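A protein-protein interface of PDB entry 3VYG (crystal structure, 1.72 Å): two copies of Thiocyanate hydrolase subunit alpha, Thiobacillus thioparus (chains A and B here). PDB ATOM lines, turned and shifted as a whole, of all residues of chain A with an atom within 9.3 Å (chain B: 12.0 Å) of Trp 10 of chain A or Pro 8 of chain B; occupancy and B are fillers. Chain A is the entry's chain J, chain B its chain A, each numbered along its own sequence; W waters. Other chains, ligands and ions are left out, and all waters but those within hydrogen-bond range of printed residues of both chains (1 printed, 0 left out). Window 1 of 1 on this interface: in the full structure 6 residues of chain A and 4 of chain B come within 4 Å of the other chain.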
ATOM      1  N   LYS A   7      -7.894 -14.234  16.987  1.00  0.00           N
ATOM      2  CA  LYS A   7      -7.290 -14.106  18.369  1.00  0.00           C
ATOM      3  C   LYS A   7      -8.251 -14.716  19.427  1.00  0.00           C
ATOM      4  O   LYS A   7      -9.506 -14.639  19.290  1.00  0.00           O
ATOM      5  CB  LYS A   7      -6.963 -12.639  18.696  1.00  0.00           C
ATOM      6  N   PRO A   8      -7.697 -15.303  20.507  1.00  0.00           N
ATOM      7  CA  PRO A   8      -8.639 -15.925  21.452  1.00  0.00           C
ATOM      8  C   PRO A   8      -9.577 -14.912  22.202  1.00  0.00           C
ATOM      9  O   PRO A   8      -9.293 -13.676  22.307  1.00  0.00           O
ATOM     10  CB  PRO A   8      -7.731 -16.750  22.388  1.00  0.00           C
ATOM     11  CG  PRO A   8      -6.390 -16.065  22.302  1.00  0.00           C
ATOM     12  CD  PRO A   8      -6.286 -15.391  20.962  1.00  0.00           C
ATOM     13  N   VAL A   9     -10.726 -15.387  22.657  1.00  0.00           N
ATOM     14  CA  VAL A   9     -11.613 -14.498  23.424  1.00  0.00           C
ATOM     15  C   VAL A   9     -11.783 -15.085  24.811  1.00  0.00           C
ATOM     16  O   VAL A   9     -12.023 -16.298  24.956  1.00  0.00           O
ATOM     17  CB  VAL A   9     -13.013 -14.330  22.790  1.00  0.00           C
ATOM     18  CG1 VAL A   9     -12.981 -13.419  21.527  1.00  0.00           C
ATOM     19  CG2 VAL A   9     -13.607 -15.702  22.511  1.00  0.00           C
ATOM     20  N   TRP A  10     -11.652 -14.222  25.827  1.00  0.00           N
ATOM     21  CA  TRP A  10     -11.656 -14.619  27.213  1.00  0.00           C
ATOM     22  C   TRP A  10     -13.052 -14.348  27.727  1.00  0.00           C
ATOM     23  O   TRP A  10     -13.611 -13.260  27.521  1.00  0.00           O
ATOM     24  CB  TRP A  10     -10.643 -13.787  28.025  1.00  0.00           C
ATOM     25  CG  TRP A  10      -9.275 -14.061  27.535  1.00  0.00           C
ATOM     26  CD1 TRP A  10      -8.554 -13.376  26.566  1.00  0.00           C
ATOM     27  CD2 TRP A  10      -8.496 -15.154  27.918  1.00  0.00           C
ATOM     28  NE1 TRP A  10      -7.345 -13.989  26.354  1.00  0.00           N
ATOM     29  CE2 TRP A  10      -7.268 -15.075  27.184  1.00  0.00           C
ATOM     30  CE3 TRP A  10      -8.662 -16.169  28.889  1.00  0.00           C
ATOM     31  CZ2 TRP A  10      -6.251 -15.995  27.346  1.00  0.00           C
ATOM     32  CZ3 TRP A  10      -7.654 -17.089  29.054  1.00  0.00           C
ATOM     33  CH2 TRP A  10      -6.437 -16.993  28.284  1.00  0.00           C
ATOM     34  N   ASP A  11     -13.628 -15.347  28.384  1.00  0.00           N
ATOM     35  CA  ASP A  11     -14.963 -15.133  28.970  1.00  0.00           C
ATOM     36  C   ASP A  11     -14.834 -14.383  30.301  1.00  0.00           C
ATOM     37  O   ASP A  11     -14.419 -14.942  31.371  1.00  0.00           O
ATOM     38  CB  ASP A  11     -15.546 -16.490  29.218  1.00  0.00           C
ATOM     39  CG  ASP A  11     -16.935 -16.427  29.758  1.00  0.00           C
ATOM     40  OD1 ASP A  11     -17.435 -15.387  30.208  1.00  0.00           O
ATOM     41  OD2 ASP A  11     -17.542 -17.474  29.708  1.00  0.00           O
ATOM     42  N   ARG A  12     -15.241 -13.120  30.294  1.00  0.00           N
ATOM     43  CA  ARG A  12     -15.148 -12.335  31.496  1.00  0.00           C
ATOM     44  C   ARG A  12     -16.391 -12.421  32.388  1.00  0.00           C
ATOM     45  O   ARG A  12     -16.461 -11.718  33.421  1.00  0.00           O
ATOM     46  CB  ARG A  12     -14.796 -10.902  31.160  1.00  0.00           C
ATOM     47  CG  ARG A  12     -13.476 -10.908  30.344  1.00  0.00           C
ATOM     48  CD  ARG A  12     -12.713  -9.674  30.504  1.00  0.00           C
ATOM     49  NE  ARG A  12     -13.423  -8.425  30.373  1.00  0.00           N
ATOM     50  CZ  ARG A  12     -13.834  -7.828  29.258  1.00  0.00           C
ATOM     51  NH1 ARG A  12     -14.392  -6.614  29.368  1.00  0.00           N
ATOM     52  NH2 ARG A  12     -13.717  -8.389  28.074  1.00  0.00           N
ATOM     53  N   THR A  13     -17.385 -13.227  31.998  1.00  0.00           N
ATOM     54  CA  THR A  13     -18.571 -13.246  32.870  1.00  0.00           C
ATOM     55  C   THR A  13     -18.699 -14.501  33.593  1.00  0.00           C
ATOM     56  O   THR A  13     -19.526 -14.623  34.519  1.00  0.00           O
ATOM     57  CB  THR A  13     -19.913 -13.027  32.044  1.00  0.00           C
ATOM     58  OG1 THR A  13     -20.042 -14.097  31.107  1.00  0.00           O
ATOM     59  CG2 THR A  13     -19.842 -11.761  31.343  1.00  0.00           C
ATOM     60  N   HIS A  14     -17.882 -15.505  33.243  1.00  0.00           N
ATOM     61  CA  HIS A  14     -18.104 -16.822  33.847  1.00  0.00           C
ATOM     62  C   HIS A  14     -18.064 -16.884  35.397  1.00  0.00           C
ATOM     63  O   HIS A  14     -18.905 -17.525  36.059  1.00  0.00           O
ATOM     64  CB  HIS A  14     -17.114 -17.857  33.247  1.00  0.00           C
ATOM     65  CG  HIS A  14     -17.091 -19.154  33.991  1.00  0.00           C
ATOM     66  ND1 HIS A  14     -17.980 -20.184  33.737  1.00  0.00           N
ATOM     67  CD2 HIS A  14     -16.293 -19.583  34.991  1.00  0.00           C
ATOM     68  CE1 HIS A  14     -17.730 -21.188  34.561  1.00  0.00           C
ATOM     69  NE2 HIS A  14     -16.725 -20.838  35.347  1.00  0.00           N
ATOM     70  N   ALA A  81      -4.940 -21.260  39.140  1.00  0.00           N
ATOM     71  CA  ALA A  81      -4.034 -20.168  38.711  1.00  0.00           C
ATOM     72  C   ALA A  81      -3.644 -20.193  37.243  1.00  0.00           C
ATOM     73  O   ALA A  81      -3.043 -19.259  36.770  1.00  0.00           O
ATOM     74  CB  ALA A  81      -2.747 -20.282  39.606  1.00  0.00           C
ATOM     75  N   PHE A  82      -4.034 -21.222  36.499  1.00  0.00           N
ATOM     76  CA  PHE A  82      -3.808 -21.256  35.044  1.00  0.00           C
ATOM     77  C   PHE A  82      -5.154 -21.309  34.315  1.00  0.00           C
ATOM     78  O   PHE A  82      -5.164 -21.555  33.126  1.00  0.00           O
ATOM     79  CB  PHE A  82      -2.933 -22.437  34.668  1.00  0.00           C
ATOM     80  CG  PHE A  82      -1.486 -22.201  35.105  1.00  0.00           C
ATOM     81  CD1 PHE A  82      -0.666 -21.443  34.285  1.00  0.00           C
ATOM     82  CD2 PHE A  82      -1.050 -22.646  36.343  1.00  0.00           C
ATOM     83  CE1 PHE A  82       0.684 -21.194  34.685  1.00  0.00           C
ATOM     84  CE2 PHE A  82       0.251 -22.374  36.788  1.00  0.00           C
ATOM     85  CZ  PHE A  82       1.087 -21.666  35.956  1.00  0.00           C
ATOM     86  N   GLY A  83      -6.224 -20.950  35.059  1.00  0.00           N
ATOM     87  CA  GLY A  83      -7.557 -20.777  34.433  1.00  0.00           C
ATOM     88  C   GLY A  83      -8.281 -22.090  34.224  1.00  0.00           C
ATOM     89  O   GLY A  83      -9.199 -22.121  33.364  1.00  0.00           O
ATOM     90  N   ASN A  84      -7.941 -23.151  34.968  1.00  0.00           N
ATOM     91  CA  ASN A  84      -8.512 -24.536  34.759  1.00  0.00           C
ATOM     92  C   ASN A  84      -9.357 -24.865  35.941  1.00  0.00           C
ATOM     93  O   ASN A  84      -8.829 -25.099  37.033  1.00  0.00           O
ATOM     94  CB  ASN A  84      -7.389 -25.553  34.576  1.00  0.00           C
ATOM     95  CG  ASN A  84      -6.459 -25.183  33.430  1.00  0.00           C
ATOM     96  OD1 ASN A  84      -5.173 -25.214  33.566  1.00  0.00           O
ATOM     97  ND2 ASN A  84      -7.035 -24.864  32.280  1.00  0.00           N
ATOM     98  N   GLU A  86     -12.224 -26.993  35.848  1.00  0.00           N
ATOM     99  CA  GLU A  86     -13.153 -28.121  35.562  1.00  0.00           C
ATOM    100  C   GLU A  86     -13.141 -29.161  36.619  1.00  0.00           C
ATOM    101  O   GLU A  86     -14.151 -29.881  36.763  1.00  0.00           O
ATOM    102  CB  GLU A  86     -12.854 -28.834  34.251  1.00  0.00           C
ATOM    103  CG  GLU A  86     -12.867 -28.009  32.986  1.00  0.00           C
ATOM    104  CD  GLU A  86     -11.667 -26.969  32.830  1.00  0.00           C
ATOM    105  OE1 GLU A  86     -10.560 -27.088  33.440  1.00  0.00           O
ATOM    106  OE2 GLU A  86     -11.896 -26.019  32.025  1.00  0.00           O
ATOM    107  N   LYS B   7     -13.504 -21.761  27.464  1.00  0.00           N
ATOM    108  CA  LYS B   7     -12.045 -21.387  27.505  1.00  0.00           C
ATOM    109  C   LYS B   7     -11.579 -20.904  26.113  1.00  0.00           C
ATOM    110  O   LYS B   7     -12.199 -21.251  25.079  1.00  0.00           O
ATOM    111  CB  LYS B   7     -11.162 -22.534  28.077  1.00  0.00           C
ATOM    112  CG  LYS B   7     -11.368 -22.707  29.660  1.00  0.00           C
ATOM    113  CD  LYS B   7     -10.135 -23.278  30.409  1.00  0.00           C
ATOM    114  CE  LYS B   7      -9.823 -24.740  30.022  1.00  0.00           C
ATOM    115  NZ  LYS B   7      -9.303 -25.530  31.183  1.00  0.00           N
ATOM    116  N   PRO B   8     -10.483 -20.100  26.061  1.00  0.00           N
ATOM    117  CA  PRO B   8     -10.059 -19.580  24.725  1.00  0.00           C
ATOM    118  C   PRO B   8      -9.567 -20.689  23.760  1.00  0.00           C
ATOM    119  O   PRO B   8      -9.145 -21.808  24.197  1.00  0.00           O
ATOM    120  CB  PRO B   8      -8.957 -18.563  25.049  1.00  0.00           C
ATOM    121  CG  PRO B   8      -8.544 -18.901  26.446  1.00  0.00           C
ATOM    122  CD  PRO B   8      -9.648 -19.597  27.172  1.00  0.00           C
ATOM    123  N   VAL B   9      -9.718 -20.424  22.472  1.00  0.00           N
ATOM    124  CA  VAL B   9      -9.103 -21.262  21.430  1.00  0.00           C
ATOM    125  C   VAL B   9      -8.137 -20.505  20.610  1.00  0.00           C
ATOM    126  O   VAL B   9      -8.320 -19.283  20.264  1.00  0.00           O
ATOM    127  CB  VAL B   9     -10.073 -22.245  20.584  1.00  0.00           C
ATOM    128  CG1 VAL B   9     -11.592 -22.260  21.092  1.00  0.00           C
ATOM    129  CG2 VAL B   9      -9.917 -22.103  19.130  1.00  0.00           C
ATOM    130  N   TRP B  10      -7.025 -21.202  20.390  1.00  0.00           N
ATOM    131  CA  TRP B  10      -5.894 -20.603  19.737  1.00  0.00           C
ATOM    132  C   TRP B  10      -5.988 -21.110  18.365  1.00  0.00           C
ATOM    133  O   TRP B  10      -6.110 -22.270  18.144  1.00  0.00           O
ATOM    134  CB  TRP B  10      -4.558 -21.068  20.410  1.00  0.00           C
ATOM    135  CG  TRP B  10      -4.554 -20.605  21.774  1.00  0.00           C
ATOM    136  CD1 TRP B  10      -4.993 -21.280  22.927  1.00  0.00           C
ATOM    137  CD2 TRP B  10      -4.154 -19.345  22.197  1.00  0.00           C
ATOM    138  NE1 TRP B  10      -4.913 -20.486  24.006  1.00  0.00           N
ATOM    139  CE2 TRP B  10      -4.347 -19.304  23.615  1.00  0.00           C
ATOM    140  CE3 TRP B  10      -3.535 -18.287  21.562  1.00  0.00           C
ATOM    141  CZ2 TRP B  10      -4.050 -18.219  24.361  1.00  0.00           C
ATOM    142  CZ3 TRP B  10      -3.228 -17.201  22.324  1.00  0.00           C
ATOM    143  CH2 TRP B  10      -3.475 -17.172  23.715  1.00  0.00           C
ATOM    144  N   ASP B  11      -5.871 -20.209  17.413  1.00  0.00           N
ATOM    145  CA  ASP B  11      -5.758 -20.581  16.010  1.00  0.00           C
ATOM    146  C   ASP B  11      -4.384 -21.106  15.721  1.00  0.00           C
ATOM    147  O   ASP B  11      -3.439 -20.318  15.778  1.00  0.00           O
ATOM    148  CB  ASP B  11      -5.908 -19.317  15.189  1.00  0.00           C
ATOM    149  CG  ASP B  11      -5.957 -19.615  13.669  1.00  0.00           C
ATOM    150  OD1 ASP B  11      -5.481 -20.672  13.239  1.00  0.00           O
ATOM    151  OD2 ASP B  11      -6.455 -18.755  12.933  1.00  0.00           O
ATOM    152  N   ARG B  12      -4.230 -22.371  15.369  1.00  0.00           N
ATOM    153  CA  ARG B  12      -2.863 -22.832  15.130  1.00  0.00           C
ATOM    154  C   ARG B  12      -2.474 -22.895  13.676  1.00  0.00           C
ATOM    155  O   ARG B  12      -1.448 -23.505  13.334  1.00  0.00           O
ATOM    156  CB  ARG B  12      -2.764 -24.209  15.722  1.00  0.00           C
ATOM    157  CG  ARG B  12      -2.591 -23.981  17.203  1.00  0.00           C
ATOM    158  CD  ARG B  12      -3.054 -25.004  18.106  1.00  0.00           C
ATOM    159  NE  ARG B  12      -2.685 -26.339  17.771  1.00  0.00           N
ATOM    160  CZ  ARG B  12      -3.445 -27.409  18.047  1.00  0.00           C
ATOM    161  NH1 ARG B  12      -3.022 -28.595  17.698  1.00  0.00           N
ATOM    162  NH2 ARG B  12      -4.590 -27.312  18.692  1.00  0.00           N
ATOM    163  N   PHE B  82       3.841 -11.227  21.604  1.00  0.00           N
ATOM    164  CA  PHE B  82       2.620 -11.356  22.412  1.00  0.00           C
ATOM    165  C   PHE B  82       1.422 -11.757  21.559  1.00  0.00           C
ATOM    166  O   PHE B  82       0.236 -11.684  22.020  1.00  0.00           O
ATOM    167  CB  PHE B  82       2.369 -10.033  23.182  1.00  0.00           C
ATOM    168  CG  PHE B  82       3.339  -9.839  24.344  1.00  0.00           C
ATOM    169  CD1 PHE B  82       3.065 -10.515  25.565  1.00  0.00           C
ATOM    170  CD2 PHE B  82       4.554  -9.122  24.238  1.00  0.00           C
ATOM    171  CE1 PHE B  82       3.946 -10.388  26.666  1.00  0.00           C
ATOM    172  CE2 PHE B  82       5.419  -9.047  25.336  1.00  0.00           C
ATOM    173  CZ  PHE B  82       5.137  -9.677  26.520  1.00  0.00           C
ATOM    174  N   GLY B  83       1.709 -12.143  20.331  1.00  0.00           N
ATOM    175  CA  GLY B  83       0.698 -12.796  19.432  1.00  0.00           C
ATOM    176  C   GLY B  83      -0.068 -11.727  18.668  1.00  0.00           C
ATOM    177  O   GLY B  83      -1.241 -12.000  18.292  1.00  0.00           O
ATOM    178  N   ASN B  84       0.480 -10.510  18.559  1.00  0.00           N
ATOM    179  CA  ASN B  84      -0.235  -9.376  17.922  1.00  0.00           C
ATOM    180  C   ASN B  84       0.452  -9.084  16.580  1.00  0.00           C
ATOM    181  O   ASN B  84       1.529  -8.499  16.557  1.00  0.00           O
ATOM    182  CB  ASN B  84      -0.132  -8.181  18.844  1.00  0.00           C
ATOM    183  CG  ASN B  84      -0.714  -8.451  20.230  1.00  0.00           C
ATOM    184  OD1 ASN B  84      -0.113  -8.138  21.312  1.00  0.00           O
ATOM    185  ND2 ASN B  84      -1.949  -8.934  20.230  1.00  0.00           N
ATOM    186  N   GLU B  86      -1.203  -7.633  13.810  1.00  0.00           N
ATOM    187  CA  GLU B  86      -2.090  -6.790  12.957  1.00  0.00           C
ATOM    188  C   GLU B  86      -1.318  -5.646  12.272  1.00  0.00           C
ATOM    189  O   GLU B  86      -1.753  -5.210  11.146  1.00  0.00           O
ATOM    190  CB  GLU B  86      -3.277  -6.243  13.778  1.00  0.00           C
ATOM    191  CG  GLU B  86      -4.178  -7.368  14.408  1.00  0.00           C
ATOM    192  CD  GLU B  86      -3.560  -7.983  15.717  1.00  0.00           C
ATOM    193  OE1 GLU B  86      -2.604  -7.377  16.325  1.00  0.00           O
ATOM    194  OE2 GLU B  86      -4.061  -9.097  16.096  1.00  0.00           O
HETATM  195  O   HOH W   1     -11.516 -17.993  21.818  1.00  0.00           O
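Of the 13 printed residues of chain A, 6 touch a printed residue of chain B. Hydrophobic or aromatic side chains of chain A within 4 Å of the printed part of chain B: Pro 8 and Trp 10. Along chain A the printed residues that touch a printed residue of chain B span positions 8 to 86. Printed residues of chain B that touch a printed residue of chain A: Lys 7, Pro 8, Val 9 and Trp 10. Hydrophobic or aromatic side chains of chain B that line the printed part of chain A: Pro 8 and Trp 10. Among the printed residues, Asp or Glu carboxylates within 4 Å of a Lys or Arg side-chain nitrogen of the other chain: Glu 86 of chain A with Lys 7 of chain B.
Among the printed residues, pairs that only touch across the chains: Pro 8 of chain A with Pro 8 of chain B, Pro 8 of chain A with Val 9 of chain B, Pro 8 of chain A with Trp 10 of chain B, Val 9 of chain A with Pro 8 of chain B, Trp 10 of chain A with Pro 8 of chain B and Gly 83 of chain A with Lys 7 of chain B.
Pro 8 of chain A touches its own counterpart, Pro 8 of chain B. Pro 8 of chain A touches Trp 10 of chain B, and with the chains exchanged Trp 10 of chain A touches Pro 8 of chain B. Gly 83 of chain A touches Lys 7 of chain B, but with the chains exchanged Lys 7 of chain A does not touch Gly 83 of chain B (5.8 Å). Asn 84 of chain A touches Lys 7 of chain B, but with the chains exchanged Lys 7 of chain A does not touch Asn 84 of chain B (6.4 Å). Positions printed for both chains: 7, 8, 9, 10, 11, 12, 82, 83, 84 and 86.
Trp 10 of chain A touches just one residue of chain B: Pro 8 (3.3 Å). Printed residues of chain A within 4 Å of Pro 8 of chain B: Pro 8 (3.4 Å), Val 9 (3.8 Å) and Trp 10 (3.3 Å). Pro 8 of chain A touches just these residues of chain B: Pro 8, Val 9 and Trp 10. No residue of chain B comes within 4 Å of Asp 11 of chain A. Arg 12 of chain A touches none of the printed residues of chain B. Gly 83 of chain A touches just one residue of chain B: Lys 7. Of chain A, only Pro 8 comes within 4 Å of Val 9 of chain B. Of the printed residues of chain B, Glu 86 of chain A touches Lys 7. Of the printed residues of chain A, Trp 10 of chain B touches Pro 8 (3.4 Å). Ala 81 of chain A touches none of the printed residues of chain B. The nearest printed residue of chain A that does not touch Pro 8 of chain B is Asp 11 of chain A (5.9 Å).
The side-chain amino group (NZ) of Lys 7 of chain B lies within salt-bridge range of the side-chain carboxylate (OE2) of Glu 86 of chain A. The side-chain amide nitrogen (ND2) of Asn 84 of chain A lies close to the side-chain amino group (NZ) of Lys 7 of chain B, 2.6 Å away.
Water W1 lies within hydrogen-bond range of the backbone NH of Val 9 of chain A (2.8 Å) and the backbone NH of Val 9 of chain B (3.1 Å).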
